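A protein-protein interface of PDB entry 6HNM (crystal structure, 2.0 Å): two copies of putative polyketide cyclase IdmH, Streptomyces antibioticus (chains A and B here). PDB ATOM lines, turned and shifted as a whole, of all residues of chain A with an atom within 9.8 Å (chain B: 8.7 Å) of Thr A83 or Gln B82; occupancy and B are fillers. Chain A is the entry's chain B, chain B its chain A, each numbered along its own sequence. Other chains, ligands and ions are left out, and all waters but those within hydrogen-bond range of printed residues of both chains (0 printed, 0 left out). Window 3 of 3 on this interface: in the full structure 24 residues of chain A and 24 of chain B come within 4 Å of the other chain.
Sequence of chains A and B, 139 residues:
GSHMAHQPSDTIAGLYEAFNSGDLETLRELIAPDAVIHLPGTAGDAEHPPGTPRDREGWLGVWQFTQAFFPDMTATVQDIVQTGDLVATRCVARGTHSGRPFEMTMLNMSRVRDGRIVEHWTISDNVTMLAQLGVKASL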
ATOM      1  N   HIS A   6     -11.629   6.647  13.480  1.00  0.00           N
ATOM      2  CA  HIS A   6     -11.265   7.370  14.734  1.00  0.00           C
ATOM      3  C   HIS A   6     -12.368   7.296  15.802  1.00  0.00           C
ATOM      4  O   HIS A   6     -12.520   8.227  16.598  1.00  0.00           O
ATOM      5  CB  HIS A   6     -10.920   8.837  14.419  1.00  0.00           C
ATOM      6  N   GLN A   7     -13.117   6.192  15.840  1.00  0.00           N
ATOM      7  CA  GLN A   7     -14.161   6.007  16.848  1.00  0.00           C
ATOM      8  C   GLN A   7     -13.615   5.750  18.252  1.00  0.00           C
ATOM      9  O   GLN A   7     -14.097   6.371  19.188  1.00  0.00           O
ATOM     10  CB  GLN A   7     -15.148   4.889  16.463  1.00  0.00           C
ATOM     11  CG  GLN A   7     -16.172   4.570  17.554  1.00  0.00           C
ATOM     12  CD  GLN A   7     -17.289   3.670  17.073  1.00  0.00           C
ATOM     13  OE1 GLN A   7     -17.079   2.786  16.240  1.00  0.00           O
ATOM     14  NE2 GLN A   7     -18.488   3.885  17.603  1.00  0.00           N
ATOM     15  N   PRO A   8     -12.648   4.819  18.417  1.00  0.00           N
ATOM     16  CA  PRO A   8     -12.164   4.520  19.776  1.00  0.00           C
ATOM     17  C   PRO A   8     -11.648   5.762  20.516  1.00  0.00           C
ATOM     18  O   PRO A   8     -11.947   5.932  21.694  1.00  0.00           O
ATOM     19  CB  PRO A   8     -11.032   3.517  19.539  1.00  0.00           C
ATOM     20  CG  PRO A   8     -11.375   2.867  18.247  1.00  0.00           C
ATOM     21  CD  PRO A   8     -11.965   3.980  17.415  1.00  0.00           C
ATOM     22  N   SER A   9     -10.913   6.623  19.812  1.00  0.00           N
ATOM     23  CA  SER A   9     -10.476   7.912  20.350  1.00  0.00           C
ATOM     24  C   SER A   9     -11.614   8.773  20.883  1.00  0.00           C
ATOM     25  O   SER A   9     -11.457   9.439  21.908  1.00  0.00           O
ATOM     26  CB  SER A   9      -9.722   8.705  19.285  1.00  0.00           C
ATOM     27  OG  SER A   9      -8.429   8.163  19.121  1.00  0.00           O
ATOM     28  N   ILE A  80      -3.365  11.893  22.889  1.00  0.00           N
ATOM     29  CA  ILE A  80      -4.110  10.689  22.611  1.00  0.00           C
ATOM     30  C   ILE A  80      -3.459  10.003  21.413  1.00  0.00           C
ATOM     31  O   ILE A  80      -3.086  10.666  20.462  1.00  0.00           O
ATOM     32  CB  ILE A  80      -5.609  10.999  22.379  1.00  0.00           C
ATOM     33  CG1 ILE A  80      -6.414   9.716  22.262  1.00  0.00           C
ATOM     34  CG2 ILE A  80      -5.834  11.908  21.169  1.00  0.00           C
ATOM     35  CD1 ILE A  80      -7.881   9.936  22.567  1.00  0.00           C
ATOM     36  N   VAL A  81      -3.279   8.690  21.493  1.00  0.00           N
ATOM     37  CA  VAL A  81      -2.785   7.904  20.367  1.00  0.00           C
ATOM     38  C   VAL A  81      -3.689   6.698  20.205  1.00  0.00           C
ATOM     39  O   VAL A  81      -4.160   6.131  21.198  1.00  0.00           O
ATOM     40  CB  VAL A  81      -1.318   7.463  20.539  1.00  0.00           C
ATOM     41  CG1 VAL A  81      -0.400   8.662  20.436  1.00  0.00           C
ATOM     42  CG2 VAL A  81      -1.097   6.770  21.870  1.00  0.00           C
ATOM     43  N   GLN A  82      -3.937   6.325  18.950  1.00  0.00           N
ATOM     44  CA  GLN A  82      -4.815   5.211  18.619  1.00  0.00           C
ATOM     45  C   GLN A  82      -4.161   4.318  17.565  1.00  0.00           C
ATOM     46  O   GLN A  82      -3.553   4.803  16.610  1.00  0.00           O
ATOM     47  CB  GLN A  82      -6.155   5.739  18.105  1.00  0.00           C
ATOM     48  CG  GLN A  82      -7.196   4.662  17.872  1.00  0.00           C
ATOM     49  CD  GLN A  82      -8.414   5.184  17.132  1.00  0.00           C
ATOM     50  OE1 GLN A  82      -9.100   6.103  17.589  1.00  0.00           O
ATOM     51  NE2 GLN A  82      -8.696   4.587  15.978  1.00  0.00           N
ATOM     52  N   THR A  83      -4.280   3.011  17.773  1.00  0.00           N
ATOM     53  CA  THR A  83      -3.898   2.002  16.784  1.00  0.00           C
ATOM     54  C   THR A  83      -4.904   0.879  16.964  1.00  0.00           C
ATOM     55  O   THR A  83      -4.897   0.205  17.991  1.00  0.00           O
ATOM     56  CB  THR A  83      -2.466   1.489  17.002  1.00  0.00           C
ATOM     57  OG1 THR A  83      -1.535   2.518  16.649  1.00  0.00           O
ATOM     58  CG2 THR A  83      -2.173   0.245  16.146  1.00  0.00           C
ATOM     59  N   GLY A  84      -5.794   0.721  15.990  1.00  0.00           N
ATOM     60  CA  GLY A  84      -6.846  -0.274  16.063  1.00  0.00           C
ATOM     61  C   GLY A  84      -7.846  -0.009  17.165  1.00  0.00           C
ATOM     62  O   GLY A  84      -8.378   1.105  17.286  1.00  0.00           O
ATOM     63  N   ASP A  85      -8.069  -1.033  17.989  1.00  0.00           N
ATOM     64  CA  ASP A  85      -8.994  -0.941  19.108  1.00  0.00           C
ATOM     65  C   ASP A  85      -8.350  -0.440  20.429  1.00  0.00           C
ATOM     66  O   ASP A  85      -9.034  -0.381  21.451  1.00  0.00           O
ATOM     67  CB  ASP A  85      -9.705  -2.288  19.312  1.00  0.00           C
ATOM     68  CG  ASP A  85      -8.787  -3.395  19.794  1.00  0.00           C
ATOM     69  OD1 ASP A  85      -7.549  -3.292  19.649  1.00  0.00           O
ATOM     70  OD2 ASP A  85      -9.326  -4.394  20.326  1.00  0.00           O
ATOM     71  N   LEU A  86      -7.070  -0.077  20.386  1.00  0.00           N
ATOM     72  CA  LEU A  86      -6.316   0.356  21.551  1.00  0.00           C
ATOM     73  C   LEU A  86      -6.083   1.868  21.507  1.00  0.00           C
ATOM     74  O   LEU A  86      -5.601   2.387  20.498  1.00  0.00           O
ATOM     75  CB  LEU A  86      -4.955  -0.334  21.603  1.00  0.00           C
ATOM     76  CG  LEU A  86      -4.751  -1.607  22.404  1.00  0.00           C
ATOM     77  CD1 LEU A  86      -3.279  -2.003  22.284  1.00  0.00           C
ATOM     78  CD2 LEU A  86      -5.168  -1.403  23.859  1.00  0.00           C
ATOM     79  N   VAL A  87      -6.424   2.554  22.605  1.00  0.00           N
ATOM     80  CA  VAL A  87      -6.227   4.010  22.746  1.00  0.00           C
ATOM     81  C   VAL A  87      -5.410   4.280  24.005  1.00  0.00           C
ATOM     82  O   VAL A  87      -5.756   3.799  25.081  1.00  0.00           O
ATOM     83  CB  VAL A  87      -7.568   4.759  22.870  1.00  0.00           C
ATOM     84  CG1 VAL A  87      -7.348   6.273  22.944  1.00  0.00           C
ATOM     85  CG2 VAL A  87      -8.490   4.429  21.712  1.00  0.00           C
ATOM     86  N   ALA A  88      -4.320   5.020  23.867  1.00  0.00           N
ATOM     87  CA  ALA A  88      -3.558   5.463  25.027  1.00  0.00           C
ATOM     88  C   ALA A  88      -3.738   6.960  25.155  1.00  0.00           C
ATOM     89  O   ALA A  88      -3.824   7.674  24.147  1.00  0.00           O
ATOM     90  CB  ALA A  88      -2.093   5.104  24.897  1.00  0.00           C
ATOM     91  N   THR A  89      -3.831   7.425  26.399  1.00  0.00           N
ATOM     92  CA  THR A  89      -4.030   8.850  26.691  1.00  0.00           C
ATOM     93  C   THR A  89      -3.129   9.313  27.816  1.00  0.00           C
ATOM     94  O   THR A  89      -2.859   8.563  28.754  1.00  0.00           O
ATOM     95  CB  THR A  89      -5.487   9.176  27.083  1.00  0.00           C
ATOM     96  OG1 THR A  89      -5.977   8.219  28.028  1.00  0.00           O
ATOM     97  CG2 THR A  89      -6.380   9.159  25.900  1.00  0.00           C
ATOM     98  N   MET A 109      -4.434   3.470  29.276  1.00  0.00           N
ATOM     99  CA  MET A 109      -4.501   2.658  28.071  1.00  0.00           C
ATOM    100  C   MET A 109      -5.830   1.926  28.106  1.00  0.00           C
ATOM    101  O   MET A 109      -6.193   1.347  29.121  1.00  0.00           O
ATOM    102  CB  MET A 109      -3.333   1.684  28.035  1.00  0.00           C
ATOM    103  CG  MET A 109      -3.343   0.704  26.858  1.00  0.00           C
ATOM    104  SD  MET A 109      -2.490   1.273  25.394  1.00  0.00           S
ATOM    105  CE  MET A 109      -0.817   1.449  26.006  1.00  0.00           C
ATOM    106  N   SER A 110      -6.553   1.973  26.996  1.00  0.00           N
ATOM    107  CA  SER A 110      -7.911   1.461  26.941  1.00  0.00           C
ATOM    108  C   SER A 110      -8.141   0.642  25.664  1.00  0.00           C
ATOM    109  O   SER A 110      -7.676   1.017  24.593  1.00  0.00           O
ATOM    110  CB  SER A 110      -8.909   2.625  26.991  1.00  0.00           C
ATOM    111  OG  SER A 110      -8.621   3.526  28.049  1.00  0.00           O
ATOM    112  N   ARG A 111      -8.850  -0.472  25.796  1.00  0.00           N
ATOM    113  CA  ARG A 111      -9.308  -1.228  24.634  1.00  0.00           C
ATOM    114  C   ARG A 111     -10.793  -0.949  24.466  1.00  0.00           C
ATOM    115  O   ARG A 111     -11.557  -1.067  25.422  1.00  0.00           O
ATOM    116  CB  ARG A 111      -9.054  -2.723  24.804  1.00  0.00           C
ATOM    117  CG  ARG A 111      -9.193  -3.490  23.491  1.00  0.00           C
ATOM    118  CD  ARG A 111      -8.899  -4.959  23.658  1.00  0.00           C
ATOM    119  NE  ARG A 111      -7.531  -5.224  24.118  1.00  0.00           N
ATOM    120  CZ  ARG A 111      -6.426  -5.207  23.363  1.00  0.00           C
ATOM    121  NH1 ARG A 111      -6.458  -4.908  22.066  1.00  0.00           N
ATOM    122  NH2 ARG A 111      -5.255  -5.511  23.911  1.00  0.00           N
ATOM    123  N   VAL A 112     -11.186  -0.554  23.258  1.00  0.00           N
ATOM    124  CA  VAL A 112     -12.576  -0.224  22.937  1.00  0.00           C
ATOM    125  C   VAL A 112     -13.114  -1.209  21.889  1.00  0.00           C
ATOM    126  O   VAL A 112     -12.435  -1.505  20.914  1.00  0.00           O
ATOM    127  CB  VAL A 112     -12.670   1.220  22.400  1.00  0.00           C
ATOM    128  CG1 VAL A 112     -14.105   1.614  22.082  1.00  0.00           C
ATOM    129  CG2 VAL A 112     -12.054   2.192  23.403  1.00  0.00           C
ATOM    130  N   GLN B   7      11.000   3.238  12.251  1.00  0.00           N
ATOM    131  CA  GLN B   7       9.725   3.840  12.764  1.00  0.00           C
ATOM    132  C   GLN B   7       9.779   4.207  14.267  1.00  0.00           C
ATOM    133  O   GLN B   7      10.571   3.631  15.030  1.00  0.00           O
ATOM    134  CB  GLN B   7       8.549   2.888  12.526  1.00  0.00           C
ATOM    135  N   PRO B   8       8.920   5.152  14.708  1.00  0.00           N
ATOM    136  CA  PRO B   8       8.910   5.504  16.136  1.00  0.00           C
ATOM    137  C   PRO B   8       8.678   4.301  17.055  1.00  0.00           C
ATOM    138  O   PRO B   8       9.339   4.186  18.070  1.00  0.00           O
ATOM    139  CB  PRO B   8       7.765   6.517  16.240  1.00  0.00           C
ATOM    140  CG  PRO B   8       7.658   7.098  14.884  1.00  0.00           C
ATOM    141  CD  PRO B   8       7.932   5.952  13.959  1.00  0.00           C
ATOM    142  N   SER B   9       7.761   3.416  16.673  1.00  0.00           N
ATOM    143  CA  SER B   9       7.550   2.135  17.366  1.00  0.00           C
ATOM    144  C   SER B   9       8.807   1.302  17.531  1.00  0.00           C
ATOM    145  O   SER B   9       8.995   0.688  18.580  1.00  0.00           O
ATOM    146  CB  SER B   9       6.495   1.299  16.643  1.00  0.00           C
ATOM    147  OG  SER B   9       5.205   1.821  16.896  1.00  0.00           O
ATOM    148  N   ASP B  10       9.651   1.274  16.497  1.00  0.00           N
ATOM    149  CA  ASP B  10      10.930   0.546  16.560  1.00  0.00           C
ATOM    150  C   ASP B  10      11.892   1.181  17.562  1.00  0.00           C
ATOM    151  O   ASP B  10      12.578   0.472  18.296  1.00  0.00           O
ATOM    152  CB  ASP B  10      11.617   0.470  15.185  1.00  0.00           C
ATOM    153  CG  ASP B  10      10.816  -0.320  14.156  1.00  0.00           C
ATOM    154  OD1 ASP B  10      10.183  -1.337  14.509  1.00  0.00           O
ATOM    155  OD2 ASP B  10      10.833   0.076  12.973  1.00  0.00           O
ATOM    156  N   THR B  11      11.936   2.513  17.587  1.00  0.00           N
ATOM    157  CA  THR B  11      12.774   3.238  18.538  1.00  0.00           C
ATOM    158  C   THR B  11      12.439   2.857  19.988  1.00  0.00           C
ATOM    159  O   THR B  11      13.342   2.600  20.793  1.00  0.00           O
ATOM    160  CB  THR B  11      12.633   4.765  18.369  1.00  0.00           C
ATOM    161  OG1 THR B  11      12.940   5.134  17.017  1.00  0.00           O
ATOM    162  CG2 THR B  11      13.556   5.509  19.328  1.00  0.00           C
ATOM    163  N   ILE B  12      11.142   2.801  20.295  1.00  0.00           N
ATOM    164  CA  ILE B  12      10.688   2.548  21.657  1.00  0.00           C
ATOM    165  C   ILE B  12      10.916   1.087  22.035  1.00  0.00           C
ATOM    166  O   ILE B  12      11.325   0.797  23.162  1.00  0.00           O
ATOM    167  CB  ILE B  12       9.209   2.956  21.860  1.00  0.00           C
ATOM    168  CG1 ILE B  12       8.996   4.435  21.488  1.00  0.00           C
ATOM    169  CG2 ILE B  12       8.771   2.737  23.304  1.00  0.00           C
ATOM    170  CD1 ILE B  12       9.888   5.442  22.188  1.00  0.00           C
ATOM    171  N   ASP B  79       1.891  -3.872  25.034  1.00  0.00           N
ATOM    172  CA  ASP B  79       1.095  -3.175  24.027  1.00  0.00           C
ATOM    173  C   ASP B  79       1.820  -1.896  23.638  1.00  0.00           C
ATOM    174  O   ASP B  79       2.464  -1.252  24.471  1.00  0.00           O
ATOM    175  CB  ASP B  79      -0.299  -2.845  24.557  1.00  0.00           C
ATOM    176  CG  ASP B  79      -1.289  -4.011  24.432  1.00  0.00           C
ATOM    177  OD1 ASP B  79      -1.333  -4.676  23.356  1.00  0.00           O
ATOM    178  OD2 ASP B  79      -2.039  -4.229  25.407  1.00  0.00           O
ATOM    179  N   ILE B  80       1.733  -1.572  22.358  1.00  0.00           N
ATOM    180  CA  ILE B  80       2.372  -0.399  21.804  1.00  0.00           C
ATOM    181  C   ILE B  80       1.393   0.227  20.825  1.00  0.00           C
ATOM    182  O   ILE B  80       0.754  -0.480  20.050  1.00  0.00           O
ATOM    183  CB  ILE B  80       3.728  -0.745  21.164  1.00  0.00           C
ATOM    184  CG1 ILE B  80       4.443   0.523  20.698  1.00  0.00           C
ATOM    185  CG2 ILE B  80       3.597  -1.726  20.012  1.00  0.00           C
ATOM    186  CD1 ILE B  80       5.931   0.344  20.529  1.00  0.00           C
ATOM    187  N   VAL B  81       1.217   1.541  20.920  1.00  0.00           N
ATOM    188  CA  VAL B  81       0.323   2.264  20.011  1.00  0.00           C
ATOM    189  C   VAL B  81       1.072   3.474  19.502  1.00  0.00           C
ATOM    190  O   VAL B  81       1.811   4.100  20.250  1.00  0.00           O
ATOM    191  CB  VAL B  81      -1.011   2.661  20.659  1.00  0.00           C
ATOM    192  CG1 VAL B  81      -1.847   1.443  20.965  1.00  0.00           C
ATOM    193  CG2 VAL B  81      -0.793   3.415  21.947  1.00  0.00           C
ATOM    194  N   GLN B  82       0.901   3.767  18.218  1.00  0.00           N
ATOM    195  CA  GLN B  82       1.622   4.839  17.545  1.00  0.00           C
ATOM    196  C   GLN B  82       0.659   5.663  16.690  1.00  0.00           C
ATOM    197  O   GLN B  82      -0.219   5.121  16.020  1.00  0.00           O
ATOM    198  CB  GLN B  82       2.742   4.260  16.676  1.00  0.00           C
ATOM    199  CG  GLN B  82       3.629   5.311  16.026  1.00  0.00           C
ATOM    200  CD  GLN B  82       4.510   4.749  14.936  1.00  0.00           C
ATOM    201  OE1 GLN B  82       5.314   3.846  15.168  1.00  0.00           O
ATOM    202  NE2 GLN B  82       4.375   5.292  13.740  1.00  0.00           N
ATOM    203  N   THR B  83       0.829   6.977  16.750  1.00  0.00           N
ATOM    204  CA  THR B  83       0.151   7.916  15.864  1.00  0.00           C
ATOM    205  C   THR B  83       1.148   9.038  15.651  1.00  0.00           C
ATOM    206  O   THR B  83       1.456   9.788  16.583  1.00  0.00           O
ATOM    207  CB  THR B  83      -1.152   8.468  16.485  1.00  0.00           C
ATOM    208  OG1 THR B  83      -2.137   7.435  16.539  1.00  0.00           O
ATOM    209  CG2 THR B  83      -1.711   9.641  15.684  1.00  0.00           C
ATOM    210  N   GLY B  84       1.678   9.123  14.433  1.00  0.00           N
ATOM    211  CA  GLY B  84       2.682  10.120  14.082  1.00  0.00           C
ATOM    212  C   GLY B  84       3.980   9.918  14.838  1.00  0.00           C
ATOM    213  O   GLY B  84       4.527   8.821  14.864  1.00  0.00           O
ATOM    214  N   ASP B  85       4.447  10.985  15.479  1.00  0.00           N
ATOM    215  CA  ASP B  85       5.684  10.959  16.256  1.00  0.00           C
ATOM    216  C   ASP B  85       5.500  10.544  17.737  1.00  0.00           C
ATOM    217  O   ASP B  85       6.469  10.551  18.501  1.00  0.00           O
ATOM    218  CB  ASP B  85       6.394  12.322  16.144  1.00  0.00           C
ATOM    219  CG  ASP B  85       5.639  13.460  16.829  1.00  0.00           C
ATOM    220  OD1 ASP B  85       4.422  13.343  17.067  1.00  0.00           O
ATOM    221  OD2 ASP B  85       6.262  14.497  17.130  1.00  0.00           O
ATOM    222  N   LEU B  86       4.273  10.191  18.133  1.00  0.00           N
ATOM    223  CA  LEU B  86       3.947   9.841  19.515  1.00  0.00           C
ATOM    224  C   LEU B  86       3.722   8.338  19.643  1.00  0.00           C
ATOM    225  O   LEU B  86       2.935   7.768  18.878  1.00  0.00           O
ATOM    226  CB  LEU B  86       2.683  10.589  19.942  1.00  0.00           C
ATOM    227  CG  LEU B  86       2.520  10.905  21.423  1.00  0.00           C
ATOM    228  CD1 LEU B  86       3.710  11.668  21.996  1.00  0.00           C
ATOM    229  CD2 LEU B  86       1.253  11.716  21.606  1.00  0.00           C
ATOM    230  N   VAL B  87       4.407   7.710  20.599  1.00  0.00           N
ATOM    231  CA  VAL B  87       4.271   6.266  20.876  1.00  0.00           C
ATOM    232  C   VAL B  87       3.934   6.063  22.350  1.00  0.00           C
ATOM    233  O   VAL B  87       4.626   6.580  23.221  1.00  0.00           O
ATOM    234  CB  VAL B  87       5.585   5.505  20.584  1.00  0.00           C
ATOM    235  CG1 VAL B  87       5.395   4.015  20.769  1.00  0.00           C
ATOM    236  CG2 VAL B  87       6.101   5.783  19.177  1.00  0.00           C
ATOM    237  N   ALA B  88       2.866   5.330  22.640  1.00  0.00           N
ATOM    238  CA  ALA B  88       2.544   4.949  24.002  1.00  0.00           C
ATOM    239  C   ALA B  88       2.797   3.460  24.154  1.00  0.00           C
ATOM    240  O   ALA B  88       2.567   2.691  23.201  1.00  0.00           O
ATOM    241  CB  ALA B  88       1.108   5.281  24.315  1.00  0.00           C
ATOM    242  N   THR B  89       3.266   3.063  25.335  1.00  0.00           N
ATOM    243  CA  THR B  89       3.499   1.655  25.646  1.00  0.00           C
ATOM    244  C   THR B  89       2.955   1.285  27.015  1.00  0.00           C
ATOM    245  O   THR B  89       3.025   2.091  27.967  1.00  0.00           O
ATOM    246  CB  THR B  89       4.995   1.291  25.625  1.00  0.00           C
ATOM    247  OG1 THR B  89       5.760   2.270  26.339  1.00  0.00           O
ATOM    248  CG2 THR B  89       5.495   1.206  24.190  1.00  0.00           C
ATOM    249  N   SER B 110       5.975   8.489  24.701  1.00  0.00           N
ATOM    250  CA  SER B 110       7.220   9.001  24.182  1.00  0.00           C
ATOM    251  C   SER B 110       7.002   9.745  22.860  1.00  0.00           C
ATOM    252  O   SER B 110       6.214   9.323  22.017  1.00  0.00           O
ATOM    253  CB  SER B 110       8.199   7.846  23.990  1.00  0.00           C
ATOM    254  OG  SER B 110       8.288   7.013  25.143  1.00  0.00           O
ATOM    255  N   VAL B 112       9.077  10.780  19.527  1.00  0.00           N
ATOM    256  CA  VAL B 112      10.292  10.412  18.795  1.00  0.00           C
ATOM    257  C   VAL B 112      10.460  11.359  17.601  1.00  0.00           C
ATOM    258  O   VAL B 112       9.503  11.619  16.878  1.00  0.00           O
ATOM    259  CB  VAL B 112      10.213   8.950  18.318  1.00  0.00           C
ATOM    260  CG1 VAL B 112      11.478   8.538  17.572  1.00  0.00           C
ATOM    261  CG2 VAL B 112       9.975   8.029  19.509  1.00  0.00           C
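Along chain A the printed residues that touch a printed residue of chain B span positions 81 to 111. Of the 19 printed residues of chain B, 7 touch a printed residue of chain A. Printed residues of chain B that touch a printed residue of chain A: Asp B79, Val B81, Gln B82, Thr B83, Leu B86, Ala B88 and Thr B89. Among the printed residues, 14 pairs touch across the chains. Among the printed residues, Asp or Glu carboxylates within 4 Å of a Lys or Arg side-chain nitrogen of the other chain: Arg A111 with Asp B79 (3.8 Å).
The side-chain hydroxyl (OG1) of Thr A83 lies within hydrogen-bond range of the backbone carbonyl oxygen (O) of Gln B82. The backbone carbonyl oxygen (O) of Gln A82 lies within hydrogen-bond range of the side-chain hydroxyl (OG1) of Thr B83. NH2 of Arg A111 lies within salt-bridge range of OD2 of Asp B79. O of Gln B82 lies close to O of Gln A82.
Val A81 touches Val B81. OG1 of Thr B83 touches CA of Val A81 (3.9 Å). CG1 of Val A81 touches CD2 of Leu B86, 3.7 Å away. Val A81 touches Ala B88. Thr A83 touches Val B81 (OG1 to CA, 3.8 Å). Leu A86 touches Asp B79. Leu A86 touches Val B81. Ala A88 touches Val B81. CB of Ala A88 touches CB of Ala B88, 3.3 Å away. Thr B89 touches Met A109 (C to CE, 3.9 Å).
Printed residues of chain B within 4 Å of Val A81: Val B81, Thr B83, Leu B86 and Ala B88. Printed residues of chain B within 4 Å of Gln A82: Gln B82 and Thr B83. Thr A83 touches just these residues of chain B: Val B81 and Gln B82. No residue of chain B comes within 4 Å of Gly A84. Printed residues of chain B within 4 Å of Arg A111: Asp B79 (3.8 Å). Val B81 touches just these residues of chain A: Val A81 (3.4 Å), Thr A83 (3.8 Å), Leu A86 (3.6 Å) and Ala A88 (3.6 Å). Gln B82 touches just these residues of chain A: Gln A82 (3.4 Å) and Thr A83 (3.0 Å). Thr B83 touches just these residues of chain A: Val A81 (3.9 Å) and Gln A82 (3.0 Å). No residue of chain A comes within 4 Å of Gly B84. Printed residues of chain A within 4 Å of Leu B86: Val A81. The nearest residue of chain A that does not touch Gln B82 is Val A81 (4.7 Å).
O of Val B81 lies within hydrogen-bond range of N of Ala B88, 2.9 Å away. The side-chain amide oxygen (OE1) of Gln B82 lies within hydrogen-bond range of the side-chain hydroxyl (OG) of Ser B9 (2.7 Å). The backbone carbonyl oxygen (O) of Ala A88 is in hydrogen-bond range of the backbone NH (N) of Val A81, 2.9 Å away. The side-chain hydroxyl (OG) of Ser A9 sits at hydrogen-bond distance from the side-chain amide oxygen (OE1) of Gln A82 (2.7 Å). NH1 of Arg A111 is in salt-bridge range of OD1 of Asp A85, at 3.1 Å.
Val A81 touches Thr B83, and with the chains exchanged Thr A83 touches Val B81. Val A81 touches Leu B86, and with the chains exchanged Leu A86 touches Val B81. Gln B82 touches its own counterpart, Gln A82. Gln A82 touches Thr B83, and with the chains exchanged Thr A83 touches Gln B82. 15 positions are printed for both chains. Of the 14 pairs that touch across the chains among the printed residues, 11 have their exchanged pair printed and touching as well.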
